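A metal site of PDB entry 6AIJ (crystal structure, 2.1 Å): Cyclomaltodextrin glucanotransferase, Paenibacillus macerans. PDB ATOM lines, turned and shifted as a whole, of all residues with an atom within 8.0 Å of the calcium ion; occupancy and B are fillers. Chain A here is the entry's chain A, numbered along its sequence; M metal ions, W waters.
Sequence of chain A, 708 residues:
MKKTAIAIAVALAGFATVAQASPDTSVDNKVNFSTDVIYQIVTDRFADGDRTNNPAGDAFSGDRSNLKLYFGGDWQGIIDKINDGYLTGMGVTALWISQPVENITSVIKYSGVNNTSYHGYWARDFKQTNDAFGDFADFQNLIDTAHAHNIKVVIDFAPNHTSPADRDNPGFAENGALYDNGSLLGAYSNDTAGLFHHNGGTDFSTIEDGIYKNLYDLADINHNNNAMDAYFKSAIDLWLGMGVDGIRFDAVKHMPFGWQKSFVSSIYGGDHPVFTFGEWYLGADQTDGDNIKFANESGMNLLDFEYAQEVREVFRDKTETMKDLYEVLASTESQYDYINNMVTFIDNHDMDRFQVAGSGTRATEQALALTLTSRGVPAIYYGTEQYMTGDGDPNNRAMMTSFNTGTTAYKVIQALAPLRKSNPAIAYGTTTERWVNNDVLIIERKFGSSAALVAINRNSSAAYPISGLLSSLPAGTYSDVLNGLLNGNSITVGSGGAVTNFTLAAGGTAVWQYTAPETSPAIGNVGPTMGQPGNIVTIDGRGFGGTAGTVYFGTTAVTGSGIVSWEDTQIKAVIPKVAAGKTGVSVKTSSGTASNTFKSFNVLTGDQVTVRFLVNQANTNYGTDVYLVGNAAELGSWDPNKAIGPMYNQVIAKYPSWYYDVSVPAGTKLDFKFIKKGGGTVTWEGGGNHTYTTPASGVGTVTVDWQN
Within 4 Å of the calcium ion: Asn 160, Ile 211, Asp 220 and His 254.
The side-chain amide nitrogen (ND2) of Asn 160 sits at hydrogen-bond distance from a ring nitrogen (ND1) of His 161 (3.2 Å).
ND1 of His 254 lies within hydrogen-bond range of O of Gly 210, 3.0 Å away.
The backbone NH (N) of Asp 220 sits close to the side-chain amide oxygen (OD1) of Asn 214.
O of Asn 160 is in hydrogen-bond range of N of Ile 221 (2.9 Å).
N of Asn 160 lies within hydrogen-bond range of SD of Met 255, at 3.7 Å.
O of Asp 220 is in hydrogen-bond range of N of His 197 (2.8 Å).
The calcium ion is bound by water W2 (2.4 Å), OD1 of Asp 220 (2.4 Å), OD1 of Asn 160 (2.4 Å), O of His 254 (2.5 Å), water W1 (2.5 Å), OD2 of Asp 220 (2.6 Å) and O of Ile 211 (2.6 Å).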
ATOM      1  N   PRO A 159      -1.090   9.959  -1.527  1.00  0.00           N
ATOM      2  CA  PRO A 159      -1.972   8.877  -1.955  1.00  0.00           C
ATOM      3  C   PRO A 159      -1.892   8.557  -3.439  1.00  0.00           C
ATOM      4  O   PRO A 159      -2.703   7.757  -3.919  1.00  0.00           O
ATOM      5  CB  PRO A 159      -3.355   9.420  -1.593  1.00  0.00           C
ATOM      6  CG  PRO A 159      -3.206  10.877  -1.906  1.00  0.00           C
ATOM      7  CD  PRO A 159      -1.801  11.248  -1.488  1.00  0.00           C
ATOM      8  N   ASN A 160      -0.960   9.166  -4.187  1.00  0.00           N
ATOM      9  CA  ASN A 160      -0.853   8.927  -5.630  1.00  0.00           C
ATOM     10  C   ASN A 160      -0.302   7.528  -5.944  1.00  0.00           C
ATOM     11  O   ASN A 160      -0.660   6.930  -6.962  1.00  0.00           O
ATOM     12  CB  ASN A 160       0.027  10.001  -6.257  1.00  0.00           C
ATOM     13  CG  ASN A 160       0.254   9.791  -7.730  1.00  0.00           C
ATOM     14  OD1 ASN A 160      -0.613  10.097  -8.536  1.00  0.00           O
ATOM     15  ND2 ASN A 160       1.442   9.309  -8.099  1.00  0.00           N
ATOM     16  N   HIS A 161       0.563   7.000  -5.089  1.00  0.00           N
ATOM     17  CA  HIS A 161       1.389   5.867  -5.448  1.00  0.00           C
ATOM     18  C   HIS A 161       1.817   5.139  -4.185  1.00  0.00           C
ATOM     19  O   HIS A 161       1.627   5.639  -3.074  1.00  0.00           O
ATOM     20  CB  HIS A 161       2.618   6.342  -6.213  1.00  0.00           C
ATOM     21  CG  HIS A 161       3.436   7.314  -5.438  1.00  0.00           C
ATOM     22  ND1 HIS A 161       3.331   8.682  -5.599  1.00  0.00           N
ATOM     23  CD2 HIS A 161       4.354   7.119  -4.456  1.00  0.00           C
ATOM     24  CE1 HIS A 161       4.170   9.281  -4.783  1.00  0.00           C
ATOM     25  NE2 HIS A 161       4.799   8.364  -4.076  1.00  0.00           N
ATOM     26  N   HIS A 197      -2.826   1.463 -11.618  1.00  0.00           N
ATOM     27  CA  HIS A 197      -2.862   1.676 -13.063  1.00  0.00           C
ATOM     28  C   HIS A 197      -1.771   0.847 -13.730  1.00  0.00           C
ATOM     29  O   HIS A 197      -0.660   0.705 -13.206  1.00  0.00           O
ATOM     30  CB  HIS A 197      -2.677   3.154 -13.425  1.00  0.00           C
ATOM     31  CG  HIS A 197      -3.869   4.009 -13.100  1.00  0.00           C
ATOM     32  ND1 HIS A 197      -3.751   5.266 -12.551  1.00  0.00           N
ATOM     33  CD2 HIS A 197      -5.205   3.784 -13.235  1.00  0.00           C
ATOM     34  CE1 HIS A 197      -4.956   5.780 -12.356  1.00  0.00           C
ATOM     35  NE2 HIS A 197      -5.860   4.900 -12.757  1.00  0.00           N
ATOM     36  N   GLU A 208      -3.429  14.937 -18.561  1.00  0.00           N
ATOM     37  CA  GLU A 208      -4.066  13.614 -18.565  1.00  0.00           C
ATOM     38  C   GLU A 208      -3.012  12.528 -18.499  1.00  0.00           C
ATOM     39  O   GLU A 208      -3.133  11.568 -17.729  1.00  0.00           O
ATOM     40  CB  GLU A 208      -4.940  13.434 -19.824  1.00  0.00           C
ATOM     41  CG  GLU A 208      -5.313  11.967 -20.069  1.00  0.00           C
ATOM     42  CD  GLU A 208      -5.913  11.713 -21.453  1.00  0.00           C
ATOM     43  OE1 GLU A 208      -5.645  12.498 -22.378  1.00  0.00           O
ATOM     44  OE2 GLU A 208      -6.644  10.709 -21.610  1.00  0.00           O
ATOM     45  N   ASP A 209      -1.948  12.685 -19.295  1.00  0.00           N
ATOM     46  CA  ASP A 209      -0.884  11.698 -19.336  1.00  0.00           C
ATOM     47  C   ASP A 209      -0.210  11.522 -17.974  1.00  0.00           C
ATOM     48  O   ASP A 209       0.207  10.411 -17.637  1.00  0.00           O
ATOM     49  CB  ASP A 209       0.139  12.091 -20.382  1.00  0.00           C
ATOM     50  CG  ASP A 209       0.896  10.901 -20.908  1.00  0.00           C
ATOM     51  OD1 ASP A 209       0.334  10.132 -21.715  1.00  0.00           O
ATOM     52  OD2 ASP A 209       2.049  10.711 -20.463  1.00  0.00           O
ATOM     53  N   GLY A 210      -0.081  12.609 -17.196  1.00  0.00           N
ATOM     54  CA  GLY A 210       0.525  12.504 -15.884  1.00  0.00           C
ATOM     55  C   GLY A 210      -0.404  12.057 -14.760  1.00  0.00           C
ATOM     56  O   GLY A 210       0.059  11.841 -13.639  1.00  0.00           O
ATOM     57  N   ILE A 211      -1.696  11.902 -15.024  1.00  0.00           N
ATOM     58  CA  ILE A 211      -2.597  11.432 -13.971  1.00  0.00           C
ATOM     59  C   ILE A 211      -2.723   9.921 -13.980  1.00  0.00           C
ATOM     60  O   ILE A 211      -2.539   9.274 -12.954  1.00  0.00           O
ATOM     61  CB  ILE A 211      -3.982  12.116 -14.084  1.00  0.00           C
ATOM     62  CG1 ILE A 211      -3.885  13.606 -13.776  1.00  0.00           C
ATOM     63  CG2 ILE A 211      -4.996  11.441 -13.145  1.00  0.00           C
ATOM     64  CD1 ILE A 211      -5.138  14.327 -14.163  1.00  0.00           C
ATOM     65  N   TYR A 212      -2.999   9.334 -15.149  1.00  0.00           N
ATOM     66  CA  TYR A 212      -3.372   7.932 -15.246  1.00  0.00           C
ATOM     67  C   TYR A 212      -2.198   7.014 -15.581  1.00  0.00           C
ATOM     68  O   TYR A 212      -2.399   5.836 -15.908  1.00  0.00           O
ATOM     69  CB  TYR A 212      -4.518   7.783 -16.264  1.00  0.00           C
ATOM     70  CG  TYR A 212      -5.761   8.560 -15.810  1.00  0.00           C
ATOM     71  CD1 TYR A 212      -6.545   8.095 -14.768  1.00  0.00           C
ATOM     72  CD2 TYR A 212      -6.119   9.783 -16.396  1.00  0.00           C
ATOM     73  CE1 TYR A 212      -7.659   8.790 -14.326  1.00  0.00           C
ATOM     74  CE2 TYR A 212      -7.250  10.478 -15.972  1.00  0.00           C
ATOM     75  CZ  TYR A 212      -8.010   9.979 -14.921  1.00  0.00           C
ATOM     76  OH  TYR A 212      -9.117  10.654 -14.469  1.00  0.00           O
ATOM     77  N   LYS A 213      -0.961   7.521 -15.465  1.00  0.00           N
ATOM     78  CA  LYS A 213       0.255   6.736 -15.691  1.00  0.00           C
ATOM     79  C   LYS A 213       1.224   6.902 -14.525  1.00  0.00           C
ATOM     80  O   LYS A 213       1.086   7.782 -13.685  1.00  0.00           O
ATOM     81  CB  LYS A 213       0.921   7.148 -16.999  1.00  0.00           C
ATOM     82  CG  LYS A 213       0.088   6.880 -18.234  1.00  0.00           C
ATOM     83  CD  LYS A 213       0.896   7.092 -19.499  1.00  0.00           C
ATOM     84  CE  LYS A 213      -0.004   6.959 -20.727  1.00  0.00           C
ATOM     85  NZ  LYS A 213       0.793   7.035 -21.975  1.00  0.00           N
ATOM     86  N   ASN A 214       2.241   6.020 -14.495  1.00  0.00           N
ATOM     87  CA  ASN A 214       3.203   6.024 -13.392  1.00  0.00           C
ATOM     88  C   ASN A 214       4.133   7.229 -13.468  1.00  0.00           C
ATOM     89  O   ASN A 214       4.562   7.656 -14.560  1.00  0.00           O
ATOM     90  CB  ASN A 214       4.023   4.732 -13.397  1.00  0.00           C
ATOM     91  CG  ASN A 214       3.183   3.472 -13.109  1.00  0.00           C
ATOM     92  OD1 ASN A 214       2.033   3.565 -12.699  1.00  0.00           O
ATOM     93  ND2 ASN A 214       3.773   2.313 -13.306  1.00  0.00           N
ATOM     94  N   LEU A 215       4.427   7.801 -12.299  1.00  0.00           N
ATOM     95  CA  LEU A 215       5.509   8.768 -12.136  1.00  0.00           C
ATOM     96  C   LEU A 215       6.828   8.008 -11.980  1.00  0.00           C
ATOM     97  O   LEU A 215       7.089   7.426 -10.921  1.00  0.00           O
ATOM     98  CB  LEU A 215       5.264   9.655 -10.914  1.00  0.00           C
ATOM     99  CG  LEU A 215       4.087  10.609 -11.053  1.00  0.00           C
ATOM    100  CD1 LEU A 215       3.798  11.321  -9.747  1.00  0.00           C
ATOM    101  CD2 LEU A 215       4.401  11.595 -12.160  1.00  0.00           C
ATOM    102  N   LEU A 218       7.060   4.621  -9.897  1.00  0.00           N
ATOM    103  CA  LEU A 218       6.161   4.554  -8.749  1.00  0.00           C
ATOM    104  C   LEU A 218       4.845   3.935  -9.175  1.00  0.00           C
ATOM    105  O   LEU A 218       4.186   4.447 -10.089  1.00  0.00           O
ATOM    106  CB  LEU A 218       5.946   5.952  -8.188  1.00  0.00           C
ATOM    107  CG  LEU A 218       7.206   6.469  -7.526  1.00  0.00           C
ATOM    108  CD1 LEU A 218       7.122   7.958  -7.346  1.00  0.00           C
ATOM    109  CD2 LEU A 218       7.464   5.742  -6.207  1.00  0.00           C
ATOM    110  N   ALA A 219       4.455   2.851  -8.495  1.00  0.00           N
ATOM    111  CA  ALA A 219       3.195   2.182  -8.803  1.00  0.00           C
ATOM    112  C   ALA A 219       2.006   3.115  -8.559  1.00  0.00           C
ATOM    113  O   ALA A 219       1.692   3.444  -7.419  1.00  0.00           O
ATOM    114  CB  ALA A 219       3.050   0.912  -7.976  1.00  0.00           C
ATOM    115  N   ASP A 220       1.315   3.498  -9.635  1.00  0.00           N
ATOM    116  CA  ASP A 220       0.244   4.477  -9.549  1.00  0.00           C
ATOM    117  C   ASP A 220      -1.041   3.843  -9.035  1.00  0.00           C
ATOM    118  O   ASP A 220      -1.515   2.837  -9.572  1.00  0.00           O
ATOM    119  CB  ASP A 220       0.020   5.098 -10.920  1.00  0.00           C
ATOM    120  CG  ASP A 220      -0.573   6.484 -10.844  1.00  0.00           C
ATOM    121  OD1 ASP A 220       0.032   7.364 -10.179  1.00  0.00           O
ATOM    122  OD2 ASP A 220      -1.639   6.706 -11.443  1.00  0.00           O
ATOM    123  N   ILE A 221      -1.606   4.440  -7.993  1.00  0.00           N
ATOM    124  CA  ILE A 221      -2.851   3.930  -7.424  1.00  0.00           C
ATOM    125  C   ILE A 221      -4.012   4.226  -8.356  1.00  0.00           C
ATOM    126  O   ILE A 221      -4.051   5.269  -9.027  1.00  0.00           O
ATOM    127  CB  ILE A 221      -3.073   4.543  -6.036  1.00  0.00           C
ATOM    128  CG1 ILE A 221      -1.958   4.090  -5.105  1.00  0.00           C
ATOM    129  CG2 ILE A 221      -4.499   4.240  -5.507  1.00  0.00           C
ATOM    130  CD1 ILE A 221      -2.241   2.757  -4.481  1.00  0.00           C
ATOM    131  N   ASN A 222      -4.957   3.298  -8.410  1.00  0.00           N
ATOM    132  CA  ASN A 222      -6.206   3.468  -9.133  1.00  0.00           C
ATOM    133  C   ASN A 222      -7.264   3.908  -8.135  1.00  0.00           C
ATOM    134  O   ASN A 222      -7.736   3.101  -7.331  1.00  0.00           O
ATOM    135  CB  ASN A 222      -6.624   2.166  -9.822  1.00  0.00           C
ATOM    136  CG  ASN A 222      -7.999   2.245 -10.454  1.00  0.00           C
ATOM    137  OD1 ASN A 222      -8.483   3.333 -10.742  1.00  0.00           O
ATOM    138  ND2 ASN A 222      -8.636   1.096 -10.650  1.00  0.00           N
ATOM    139  N   HIS A 223      -7.633   5.183  -8.158  1.00  0.00           N
ATOM    140  CA  HIS A 223      -8.634   5.654  -7.204  1.00  0.00           C
ATOM    141  C   HIS A 223     -10.058   5.471  -7.703  1.00  0.00           C
ATOM    142  O   HIS A 223     -11.005   5.781  -6.967  1.00  0.00           O
ATOM    143  CB  HIS A 223      -8.397   7.130  -6.836  1.00  0.00           C
ATOM    144  CG  HIS A 223      -7.018   7.417  -6.333  1.00  0.00           C
ATOM    145  ND1 HIS A 223      -6.023   7.948  -7.120  1.00  0.00           N
ATOM    146  CD2 HIS A 223      -6.476   7.250  -5.094  1.00  0.00           C
ATOM    147  CE1 HIS A 223      -4.918   8.084  -6.408  1.00  0.00           C
ATOM    148  NE2 HIS A 223      -5.167   7.672  -5.169  1.00  0.00           N
ATOM    149  N   ALA A 251       1.697  15.801  -5.036  1.00  0.00           N
ATOM    150  CA  ALA A 251       1.519  15.450  -6.444  1.00  0.00           C
ATOM    151  C   ALA A 251       0.082  15.645  -6.924  1.00  0.00           C
ATOM    152  O   ALA A 251      -0.416  14.834  -7.703  1.00  0.00           O
ATOM    153  CB  ALA A 251       1.970  14.017  -6.720  1.00  0.00           C
ATOM    154  N   LYS A 253      -1.239  17.399  -9.024  1.00  0.00           N
ATOM    155  CA  LYS A 253      -1.306  17.466 -10.479  1.00  0.00           C
ATOM    156  C   LYS A 253      -1.493  16.084 -11.128  1.00  0.00           C
ATOM    157  O   LYS A 253      -1.982  15.993 -12.251  1.00  0.00           O
ATOM    158  CB  LYS A 253      -0.021  18.113 -10.997  1.00  0.00           C
ATOM    159  CG  LYS A 253       0.086  18.479 -12.458  1.00  0.00           C
ATOM    160  CD  LYS A 253       1.287  19.428 -12.601  1.00  0.00           C
ATOM    161  CE  LYS A 253       1.571  19.879 -14.018  1.00  0.00           C
ATOM    162  NZ  LYS A 253       2.726  20.839 -13.992  1.00  0.00           N
ATOM    163  N   HIS A 254      -1.107  15.020 -10.425  1.00  0.00           N
ATOM    164  CA  HIS A 254      -1.073  13.672 -10.986  1.00  0.00           C
ATOM    165  C   HIS A 254      -2.153  12.770 -10.415  1.00  0.00           C
ATOM    166  O   HIS A 254      -2.016  11.550 -10.504  1.00  0.00           O
ATOM    167  CB  HIS A 254       0.304  13.071 -10.757  1.00  0.00           C
ATOM    168  CG  HIS A 254       1.406  13.940 -11.251  1.00  0.00           C
ATOM    169  ND1 HIS A 254       1.707  14.060 -12.588  1.00  0.00           N
ATOM    170  CD2 HIS A 254       2.222  14.797 -10.597  1.00  0.00           C
ATOM    171  CE1 HIS A 254       2.687  14.922 -12.735  1.00  0.00           C
ATOM    172  NE2 HIS A 254       3.026  15.376 -11.544  1.00  0.00           N
ATOM    173  N   MET A 255      -3.203  13.342  -9.829  1.00  0.00           N
ATOM    174  CA  MET A 255      -4.386  12.583  -9.425  1.00  0.00           C
ATOM    175  C   MET A 255      -5.619  13.250 -10.000  1.00  0.00           C
ATOM    176  O   MET A 255      -5.588  14.438 -10.306  1.00  0.00           O
ATOM    177  CB  MET A 255      -4.507  12.478  -7.897  1.00  0.00           C
ATOM    178  CG  MET A 255      -3.502  11.531  -7.278  1.00  0.00           C
ATOM    179  SD  MET A 255      -3.477  11.560  -5.466  1.00  0.00           S
ATOM    180  CE  MET A 255      -2.851  13.242  -5.122  1.00  0.00           C
ATOM    181  N   PRO A 256      -6.709  12.501 -10.203  1.00  0.00           N
ATOM    182  CA  PRO A 256      -7.920  13.124 -10.778  1.00  0.00           C
ATOM    183  C   PRO A 256      -8.438  14.235  -9.873  1.00  0.00           C
ATOM    184  O   PRO A 256      -8.562  14.072  -8.654  1.00  0.00           O
ATOM    185  CB  PRO A 256      -8.912  11.947 -10.859  1.00  0.00           C
ATOM    186  CG  PRO A 256      -8.053  10.728 -10.917  1.00  0.00           C
ATOM    187  CD  PRO A 256      -6.847  11.039 -10.064  1.00  0.00           C
HETATM  188 CA    CA M   1      -1.600   9.131 -10.540  1.00  0.00          CA
HETATM  189  O   HOH W   1      -4.058   9.219 -10.618  1.00  0.00           O
HETATM  190  O   HOH W   2       0.291   9.722 -11.934  1.00  0.00           O
